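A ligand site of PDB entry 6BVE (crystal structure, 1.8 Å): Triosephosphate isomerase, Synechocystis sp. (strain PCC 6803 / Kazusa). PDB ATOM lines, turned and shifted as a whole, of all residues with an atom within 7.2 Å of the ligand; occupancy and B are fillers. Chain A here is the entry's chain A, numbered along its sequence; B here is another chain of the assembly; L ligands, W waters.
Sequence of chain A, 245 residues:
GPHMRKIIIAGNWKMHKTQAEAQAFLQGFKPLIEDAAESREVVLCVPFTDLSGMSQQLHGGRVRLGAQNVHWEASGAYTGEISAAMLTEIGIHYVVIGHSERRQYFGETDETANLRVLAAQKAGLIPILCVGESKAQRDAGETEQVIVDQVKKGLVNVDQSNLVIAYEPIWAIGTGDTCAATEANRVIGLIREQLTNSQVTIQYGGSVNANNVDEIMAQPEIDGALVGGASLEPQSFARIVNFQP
Water W1 lies within hydrogen-bond range of an oxygen (O4) of the ligand (2.8 Å) and the side-chain amino group of Lys 14 (2.9 Å). Water W4 lies within hydrogen-bond range of the backbone carbonyl oxygen of Val 208 (2.7 Å), an oxygen (O2) of the ligand (2.8 Å), the backbone NH of Ala 230 (2.9 Å) and the backbone NH of Gly 229 (3.4 Å).
Residues that only touch the ligand: Ala 172, Ile 173, Gly 206, Leu 226 and Val 227. Within 4 Å of the ligand: Asn 12, Lys 14, His 99, Glu 168, Ala 172, Ile 173, Gly 174, Gly 206, Ser 207, Leu 226, Val 227, Gly 228 and Gly 229. Along chain A the residues within 4 Å of the ligand span positions 12 to 229. The nearest printed residue that does not touch the ligand is Val 208 (4.1 Å).
An oxygen (O2) of the ligand sits at hydrogen-bond distance from the backbone NH of Gly 228. The side-chain amide nitrogen of Asn 12 sits at hydrogen-bond distance from an oxygen (O5) of the ligand (3.3 Å). The side-chain carboxylate of Glu 168 lies close to an oxygen (O5) of the ligand (2.8 Å). O4 of the ligand is in hydrogen-bond range of N of Gly 229, at 2.9 Å. O3 of the ligand lies within hydrogen-bond range of N of Gly 174 (2.8 Å). An oxygen (O6) of the ligand is in salt-bridge range of the side-chain amino group (NZ) of Lys 14 (2.8 Å). N of Ser 207 sits at hydrogen-bond distance from O3 of the ligand (2.7 Å). An oxygen (O6) of the ligand lies within hydrogen-bond range of a ring nitrogen (NE2) of His 99, 2.7 Å away.
The side-chain hydroxyl of Ser 207 is in hydrogen-bond range of the backbone carbonyl oxygen of Ala 172 (2.7 Å). The backbone carbonyl oxygen of Val 227 sits at hydrogen-bond distance from the backbone NH of Asn 12 (2.7 Å). The backbone carbonyl oxygen (O) of Gly 206 sits at hydrogen-bond distance from the side-chain hydroxyl (OH) of Tyr 204, at 2.8 Å. The backbone NH (N) of Val 227 sits at hydrogen-bond distance from the backbone carbonyl oxygen (O) of Ala 10. OG of Ser 207 lies within hydrogen-bond range of N of Gly 176. OE1 of Glu 168 lies within hydrogen-bond range of NE2 of His 99, at 3.3 Å. O of Val 227 is in hydrogen-bond range of OG of Ser 231. The backbone carbonyl oxygen (O) of Gly 228 is in hydrogen-bond range of the side-chain hydroxyl (OG) of Ser 231 (2.8 Å).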
ATOM      1  N   ALA A  10      -8.445 -22.029  18.511  1.00  0.00           N
ATOM      2  CA  ALA A  10      -9.462 -22.871  17.889  1.00  0.00           C
ATOM      3  C   ALA A  10      -9.135 -23.050  16.417  1.00  0.00           C
ATOM      4  O   ALA A  10      -8.811 -22.079  15.721  1.00  0.00           O
ATOM      5  CB  ALA A  10     -10.863 -22.267  18.055  1.00  0.00           C
ATOM      6  N   GLY A  11      -9.207 -24.293  15.952  1.00  0.00           N
ATOM      7  CA  GLY A  11      -8.983 -24.606  14.552  1.00  0.00           C
ATOM      8  C   GLY A  11     -10.315 -24.819  13.870  1.00  0.00           C
ATOM      9  O   GLY A  11     -11.118 -25.642  14.278  1.00  0.00           O
ATOM     10  N   ASN A  12     -10.536 -24.066  12.803  1.00  0.00           N
ATOM     11  CA  ASN A  12     -11.721 -24.236  11.992  1.00  0.00           C
ATOM     12  C   ASN A  12     -11.300 -25.010  10.750  1.00  0.00           C
ATOM     13  O   ASN A  12     -10.798 -24.422   9.790  1.00  0.00           O
ATOM     14  CB  ASN A  12     -12.328 -22.882  11.634  1.00  0.00           C
ATOM     15  CG  ASN A  12     -13.557 -23.010  10.742  1.00  0.00           C
ATOM     16  OD1 ASN A  12     -14.038 -24.119  10.499  1.00  0.00           O
ATOM     17  ND2 ASN A  12     -14.067 -21.871  10.243  1.00  0.00           N
ATOM     18  N   TRP A  13     -11.528 -26.326  10.757  1.00  0.00           N
ATOM     19  CA  TRP A  13     -11.180 -27.147   9.592  1.00  0.00           C
ATOM     20  C   TRP A  13     -12.024 -26.833   8.366  1.00  0.00           C
ATOM     21  O   TRP A  13     -11.658 -27.238   7.257  1.00  0.00           O
ATOM     22  CB  TRP A  13     -11.359 -28.626   9.922  1.00  0.00           C
ATOM     23  CG  TRP A  13     -10.236 -29.208  10.695  1.00  0.00           C
ATOM     24  CD1 TRP A  13      -9.060 -28.596  11.025  1.00  0.00           C
ATOM     25  CD2 TRP A  13     -10.187 -30.540  11.225  1.00  0.00           C
ATOM     26  NE1 TRP A  13      -8.263 -29.484  11.740  1.00  0.00           N
ATOM     27  CE2 TRP A  13      -8.930 -30.679  11.868  1.00  0.00           C
ATOM     28  CE3 TRP A  13     -11.062 -31.624  11.207  1.00  0.00           C
ATOM     29  CZ2 TRP A  13      -8.554 -31.865  12.496  1.00  0.00           C
ATOM     30  CZ3 TRP A  13     -10.699 -32.786  11.847  1.00  0.00           C
ATOM     31  CH2 TRP A  13      -9.450 -32.907  12.480  1.00  0.00           C
ATOM     32  N   LYS A  14     -13.160 -26.169   8.550  1.00  0.00           N
ATOM     33  CA  LYS A  14     -14.110 -25.911   7.439  1.00  0.00           C
ATOM     34  C   LYS A  14     -14.497 -27.255   6.823  1.00  0.00           C
ATOM     35  O   LYS A  14     -14.634 -28.257   7.543  1.00  0.00           O
ATOM     36  CB  LYS A  14     -13.524 -24.894   6.473  1.00  0.00           C
ATOM     37  CG  LYS A  14     -13.146 -23.610   7.190  1.00  0.00           C
ATOM     38  CD  LYS A  14     -12.842 -22.462   6.230  1.00  0.00           C
ATOM     39  CE  LYS A  14     -12.386 -21.230   7.007  1.00  0.00           C
ATOM     40  NZ  LYS A  14     -12.136 -20.033   6.113  1.00  0.00           N
ATOM     41  N   VAL A  96     -19.083 -23.012  16.267  1.00  0.00           N
ATOM     42  CA  VAL A  96     -18.881 -21.804  15.482  1.00  0.00           C
ATOM     43  C   VAL A  96     -20.211 -21.352  14.918  1.00  0.00           C
ATOM     44  O   VAL A  96     -20.943 -22.141  14.309  1.00  0.00           O
ATOM     45  CB  VAL A  96     -17.866 -22.057  14.357  1.00  0.00           C
ATOM     46  CG1 VAL A  96     -17.650 -20.781  13.590  1.00  0.00           C
ATOM     47  CG2 VAL A  96     -16.547 -22.572  14.962  1.00  0.00           C
ATOM     48  N   HIS A  99     -20.260 -17.787  10.951  1.00  0.00           N
ATOM     49  CA  HIS A  99     -19.075 -17.674  10.134  1.00  0.00           C
ATOM     50  C   HIS A  99     -19.388 -16.965   8.819  1.00  0.00           C
ATOM     51  O   HIS A  99     -20.445 -17.186   8.220  1.00  0.00           O
ATOM     52  CB  HIS A  99     -18.479 -19.052   9.832  1.00  0.00           C
ATOM     53  CG  HIS A  99     -17.092 -18.963   9.330  1.00  0.00           C
ATOM     54  ND1 HIS A  99     -16.786 -18.766   7.995  1.00  0.00           N
ATOM     55  CD2 HIS A  99     -15.910 -18.973   9.992  1.00  0.00           C
ATOM     56  CE1 HIS A  99     -15.477 -18.672   7.860  1.00  0.00           C
ATOM     57  NE2 HIS A  99     -14.925 -18.802   9.046  1.00  0.00           N
ATOM     58  N   SER A 100     -18.443 -16.134   8.368  1.00  0.00           N
ATOM     59  CA  SER A 100     -18.649 -15.342   7.150  1.00  0.00           C
ATOM     60  C   SER A 100     -19.090 -16.205   5.985  1.00  0.00           C
ATOM     61  O   SER A 100     -19.901 -15.774   5.152  1.00  0.00           O
ATOM     62  CB  SER A 100     -17.366 -14.586   6.801  1.00  0.00           C
ATOM     63  OG  SER A 100     -17.469 -13.947   5.525  1.00  0.00           O
ATOM     64  N   GLU A 101     -18.594 -17.448   5.906  1.00  0.00           N
ATOM     65  CA  GLU A 101     -18.936 -18.278   4.751  1.00  0.00           C
ATOM     66  C   GLU A 101     -20.406 -18.672   4.765  1.00  0.00           C
ATOM     67  O   GLU A 101     -21.029 -18.798   3.704  1.00  0.00           O
ATOM     68  CB  GLU A 101     -18.030 -19.517   4.706  1.00  0.00           C
ATOM     69  CG  GLU A 101     -16.650 -19.156   4.214  1.00  0.00           C
ATOM     70  CD  GLU A 101     -15.531 -19.992   4.819  1.00  0.00           C
ATOM     71  OE1 GLU A 101     -15.793 -21.066   5.392  1.00  0.00           O
ATOM     72  OE2 GLU A 101     -14.369 -19.561   4.713  1.00  0.00           O
ATOM     73  N   CYS A 130     -19.030 -15.200  15.118  1.00  0.00           N
ATOM     74  CA  CYS A 130     -18.082 -14.595  14.170  1.00  0.00           C
ATOM     75  C   CYS A 130     -18.659 -13.291  13.634  1.00  0.00           C
ATOM     76  O   CYS A 130     -19.822 -13.243  13.233  1.00  0.00           O
ATOM     77  CB  CYS A 130     -17.811 -15.540  13.002  1.00  0.00           C
ATOM     78  SG  CYS A 130     -17.029 -17.082  13.512  1.00  0.00           S
ATOM     79  N   ALA A 166     -15.279 -14.057  17.688  1.00  0.00           N
ATOM     80  CA  ALA A 166     -14.156 -14.067  16.768  1.00  0.00           C
ATOM     81  C   ALA A 166     -14.346 -12.939  15.762  1.00  0.00           C
ATOM     82  O   ALA A 166     -15.338 -12.932  15.023  1.00  0.00           O
ATOM     83  CB  ALA A 166     -14.022 -15.416  16.055  1.00  0.00           C
ATOM     84  N   GLU A 168     -13.244 -11.639  12.448  1.00  0.00           N
ATOM     85  CA  GLU A 168     -12.587 -12.169  11.255  1.00  0.00           C
ATOM     86  C   GLU A 168     -12.884 -11.216  10.121  1.00  0.00           C
ATOM     87  O   GLU A 168     -13.889 -11.381   9.410  1.00  0.00           O
ATOM     88  CB  GLU A 168     -13.062 -13.585  10.935  1.00  0.00           C
ATOM     89  CG  GLU A 168     -12.760 -14.599  12.039  1.00  0.00           C
ATOM     90  CD  GLU A 168     -12.844 -16.048  11.565  1.00  0.00           C
ATOM     91  OE1 GLU A 168     -13.926 -16.436  11.067  1.00  0.00           O
ATOM     92  OE2 GLU A 168     -11.840 -16.814  11.723  1.00  0.00           O
ATOM     93  N   ALA A 172      -9.493 -10.911   5.103  1.00  0.00           N
ATOM     94  CA  ALA A 172      -8.344 -11.621   5.620  1.00  0.00           C
ATOM     95  C   ALA A 172      -8.539 -13.129   5.618  1.00  0.00           C
ATOM     96  O   ALA A 172      -7.585 -13.871   5.880  1.00  0.00           O
ATOM     97  CB  ALA A 172      -8.015 -11.149   7.048  1.00  0.00           C
ATOM     98  N   ILE A 173      -9.758 -13.590   5.338  1.00  0.00           N
ATOM     99  CA  ILE A 173     -10.092 -15.013   5.440  1.00  0.00           C
ATOM    100  C   ILE A 173      -9.617 -15.751   4.191  1.00  0.00           C
ATOM    101  O   ILE A 173     -10.120 -15.507   3.083  1.00  0.00           O
ATOM    102  CB  ILE A 173     -11.596 -15.205   5.663  1.00  0.00           C
ATOM    103  CG1 ILE A 173     -12.005 -14.570   7.010  1.00  0.00           C
ATOM    104  CG2 ILE A 173     -11.958 -16.689   5.630  1.00  0.00           C
ATOM    105  CD1 ILE A 173     -13.487 -14.604   7.275  1.00  0.00           C
ATOM    106  N   GLY A 174      -8.662 -16.650   4.376  1.00  0.00           N
ATOM    107  CA  GLY A 174      -8.193 -17.493   3.297  1.00  0.00           C
ATOM    108  C   GLY A 174      -7.371 -16.804   2.248  1.00  0.00           C
ATOM    109  O   GLY A 174      -6.984 -17.449   1.270  1.00  0.00           O
ATOM    110  N   THR A 175      -7.063 -15.522   2.430  1.00  0.00           N
ATOM    111  CA  THR A 175      -6.388 -14.729   1.401  1.00  0.00           C
ATOM    112  C   THR A 175      -4.901 -14.589   1.647  1.00  0.00           C
ATOM    113  O   THR A 175      -4.180 -14.156   0.735  1.00  0.00           O
ATOM    114  CB  THR A 175      -6.978 -13.325   1.343  1.00  0.00           C
ATOM    115  OG1 THR A 175      -6.892 -12.773   2.666  1.00  0.00           O
ATOM    116  CG2 THR A 175      -8.451 -13.353   0.892  1.00  0.00           C
ATOM    117  N   GLY A 176      -4.424 -14.896   2.853  1.00  0.00           N
ATOM    118  CA  GLY A 176      -3.067 -14.579   3.227  1.00  0.00           C
ATOM    119  C   GLY A 176      -2.863 -13.136   3.623  1.00  0.00           C
ATOM    120  O   GLY A 176      -1.741 -12.778   4.051  1.00  0.00           O
ATOM    121  N   TYR A 204      -9.018 -13.290  17.253  1.00  0.00           N
ATOM    122  CA  TYR A 204      -8.822 -12.811  15.891  1.00  0.00           C
ATOM    123  C   TYR A 204      -8.833 -14.023  14.965  1.00  0.00           C
ATOM    124  O   TYR A 204      -8.268 -15.065  15.288  1.00  0.00           O
ATOM    125  CB  TYR A 204      -7.498 -12.055  15.744  1.00  0.00           C
ATOM    126  CG  TYR A 204      -7.181 -11.794  14.295  1.00  0.00           C
ATOM    127  CD1 TYR A 204      -7.812 -10.771  13.601  1.00  0.00           C
ATOM    128  CD2 TYR A 204      -6.297 -12.615  13.599  1.00  0.00           C
ATOM    129  CE1 TYR A 204      -7.563 -10.543  12.246  1.00  0.00           C
ATOM    130  CE2 TYR A 204      -6.044 -12.398  12.235  1.00  0.00           C
ATOM    131  CZ  TYR A 204      -6.666 -11.355  11.576  1.00  0.00           C
ATOM    132  OH  TYR A 204      -6.418 -11.150  10.223  1.00  0.00           O
ATOM    133  N   GLY A 205      -9.475 -13.888  13.815  1.00  0.00           N
ATOM    134  CA  GLY A 205      -9.326 -14.869  12.758  1.00  0.00           C
ATOM    135  C   GLY A 205      -9.033 -14.184  11.436  1.00  0.00           C
ATOM    136  O   GLY A 205      -9.426 -13.052  11.204  1.00  0.00           O
ATOM    137  N   GLY A 206      -8.315 -14.904  10.567  1.00  0.00           N
ATOM    138  CA  GLY A 206      -8.098 -14.395   9.223  1.00  0.00           C
ATOM    139  C   GLY A 206      -6.649 -14.505   8.844  1.00  0.00           C
ATOM    140  O   GLY A 206      -5.868 -13.592   9.080  1.00  0.00           O
ATOM    141  N   SER A 207      -6.274 -15.656   8.293  1.00  0.00           N
ATOM    142  CA  SER A 207      -4.893 -15.942   7.884  1.00  0.00           C
ATOM    143  C   SER A 207      -3.924 -15.891   9.069  1.00  0.00           C
ATOM    144  O   SER A 207      -2.780 -15.429   8.924  1.00  0.00           O
ATOM    145  CB  SER A 207      -4.449 -15.000   6.768  1.00  0.00           C
ATOM    146  OG  SER A 207      -5.246 -15.190   5.609  1.00  0.00           O
ATOM    147  N   VAL A 208      -4.370 -16.371  10.230  1.00  0.00           N
ATOM    148  CA  VAL A 208      -3.428 -16.703  11.299  1.00  0.00           C
ATOM    149  C   VAL A 208      -2.567 -17.890  10.881  1.00  0.00           C
ATOM    150  O   VAL A 208      -3.069 -18.899  10.369  1.00  0.00           O
ATOM    151  CB  VAL A 208      -4.174 -17.008  12.615  1.00  0.00           C
ATOM    152  CG1 VAL A 208      -3.175 -17.423  13.727  1.00  0.00           C
ATOM    153  CG2 VAL A 208      -4.992 -15.810  13.048  1.00  0.00           C
ATOM    154  N   ASN A 209      -1.260 -17.795  11.120  1.00  0.00           N
ATOM    155  CA  ASN A 209      -0.388 -18.908  10.818  1.00  0.00           C
ATOM    156  C   ASN A 209       0.670 -19.005  11.914  1.00  0.00           C
ATOM    157  O   ASN A 209       0.698 -18.199  12.849  1.00  0.00           O
ATOM    158  CB  ASN A 209       0.217 -18.764   9.411  1.00  0.00           C
ATOM    159  CG  ASN A 209       0.986 -17.472   9.229  1.00  0.00           C
ATOM    160  OD1 ASN A 209       1.892 -17.182  10.007  1.00  0.00           O
ATOM    161  ND2 ASN A 209       0.640 -16.707   8.189  1.00  0.00           N
ATOM    162  N   LEU A 226      -8.982 -17.971  15.802  1.00  0.00           N
ATOM    163  CA  LEU A 226      -9.787 -18.925  15.055  1.00  0.00           C
ATOM    164  C   LEU A 226      -9.033 -19.136  13.755  1.00  0.00           C
ATOM    165  O   LEU A 226      -8.882 -18.207  12.959  1.00  0.00           O
ATOM    166  CB  LEU A 226     -11.205 -18.401  14.795  1.00  0.00           C
ATOM    167  CG  LEU A 226     -12.193 -19.390  14.168  1.00  0.00           C
ATOM    168  CD1 LEU A 226     -12.289 -20.658  14.999  1.00  0.00           C
ATOM    169  CD2 LEU A 226     -13.590 -18.750  14.056  1.00  0.00           C
ATOM    170  N   VAL A 227      -8.499 -20.340  13.565  1.00  0.00           N
ATOM    171  CA  VAL A 227      -7.470 -20.604  12.571  1.00  0.00           C
ATOM    172  C   VAL A 227      -8.067 -21.510  11.511  1.00  0.00           C
ATOM    173  O   VAL A 227      -8.490 -22.628  11.822  1.00  0.00           O
ATOM    174  CB  VAL A 227      -6.226 -21.255  13.207  1.00  0.00           C
ATOM    175  CG1 VAL A 227      -5.165 -21.443  12.177  1.00  0.00           C
ATOM    176  CG2 VAL A 227      -5.703 -20.398  14.386  1.00  0.00           C
ATOM    177  N   GLY A 228      -8.061 -21.049  10.259  1.00  0.00           N
ATOM    178  CA  GLY A 228      -8.561 -21.871   9.157  1.00  0.00           C
ATOM    179  C   GLY A 228      -7.495 -22.757   8.528  1.00  0.00           C
ATOM    180  O   GLY A 228      -7.197 -23.850   9.032  1.00  0.00           O
ATOM    181  N   GLY A 229      -6.908 -22.289   7.429  1.00  0.00           N
ATOM    182  CA  GLY A 229      -6.009 -23.129   6.664  1.00  0.00           C
ATOM    183  C   GLY A 229      -4.846 -23.653   7.485  1.00  0.00           C
ATOM    184  O   GLY A 229      -4.439 -24.813   7.331  1.00  0.00           O
ATOM    185  N   ALA A 230      -4.323 -22.841   8.396  1.00  0.00           N
ATOM    186  CA  ALA A 230      -3.174 -23.271   9.190  1.00  0.00           C
ATOM    187  C   ALA A 230      -3.546 -24.242  10.298  1.00  0.00           C
ATOM    188  O   ALA A 230      -2.640 -24.734  11.008  1.00  0.00           O
ATOM    189  CB  ALA A 230      -2.456 -22.051   9.776  1.00  0.00           C
ATOM    190  N   SER A 231      -4.822 -24.565  10.473  1.00  0.00           N
ATOM    191  CA  SER A 231      -5.218 -25.603  11.423  1.00  0.00           C
ATOM    192  C   SER A 231      -5.341 -26.979  10.795  1.00  0.00           C
ATOM    193  O   SER A 231      -5.648 -27.927  11.505  1.00  0.00           O
ATOM    194  CB  SER A 231      -6.549 -25.227  12.101  1.00  0.00           C
ATOM    195  OG  SER A 231      -7.659 -25.474  11.248  1.00  0.00           O
ATOM    196  N   ALA B  77     -13.337 -24.028   1.698  1.00  0.00           N
ATOM    197  CA  ALA B  77     -13.645 -23.006   2.700  1.00  0.00           C
ATOM    198  C   ALA B  77     -15.160 -22.787   2.733  1.00  0.00           C
ATOM    199  O   ALA B  77     -15.696 -21.765   2.283  1.00  0.00           O
ATOM    200  CB  ALA B  77     -12.906 -21.707   2.385  1.00  0.00           C
ATOM    201  N   THR B  79     -17.448 -23.435   5.703  1.00  0.00           N
ATOM    202  CA  THR B  79     -17.711 -23.767   7.088  1.00  0.00           C
ATOM    203  C   THR B  79     -19.145 -24.276   7.244  1.00  0.00           C
ATOM    204  O   THR B  79     -20.084 -23.669   6.729  1.00  0.00           O
ATOM    205  CB  THR B  79     -17.477 -22.533   7.954  1.00  0.00           C
ATOM    206  OG1 THR B  79     -16.088 -22.185   7.907  1.00  0.00           O
ATOM    207  CG2 THR B  79     -17.894 -22.795   9.401  1.00  0.00           C
HETATM  208  P1  LIG L   1      -8.129 -18.726   7.533  1.00  0.00           P
HETATM  209  O1  LIG L   1      -9.657 -18.960   7.926  1.00  0.00           O
HETATM  210  O2  LIG L   1      -7.281 -18.903   8.787  1.00  0.00           O
HETATM  211  O3  LIG L   1      -8.024 -17.305   7.049  1.00  0.00           O
HETATM  212  O4  LIG L   1      -7.755 -19.682   6.401  1.00  0.00           O
HETATM  213  C1  LIG L   1     -10.078 -18.548   9.207  1.00  0.00           C
HETATM  214  C2  LIG L   1     -11.568 -18.719   9.298  1.00  0.00           C
HETATM  215  O5  LIG L   1     -12.068 -19.198  10.344  1.00  0.00           O
HETATM  216  O6  LIG L   1     -12.302 -18.375   8.339  1.00  0.00           O
HETATM  217  O   HOH W   1      -9.680 -20.851   4.786  1.00  0.00           O
HETATM  218  O   HOH W   2      -5.855 -20.115   4.627  1.00  0.00           O
HETATM  219  O   HOH W   3      -7.117 -17.478  10.897  1.00  0.00           O
HETATM  220  O   HOH W   4      -4.731 -20.004   8.613  1.00  0.00           O
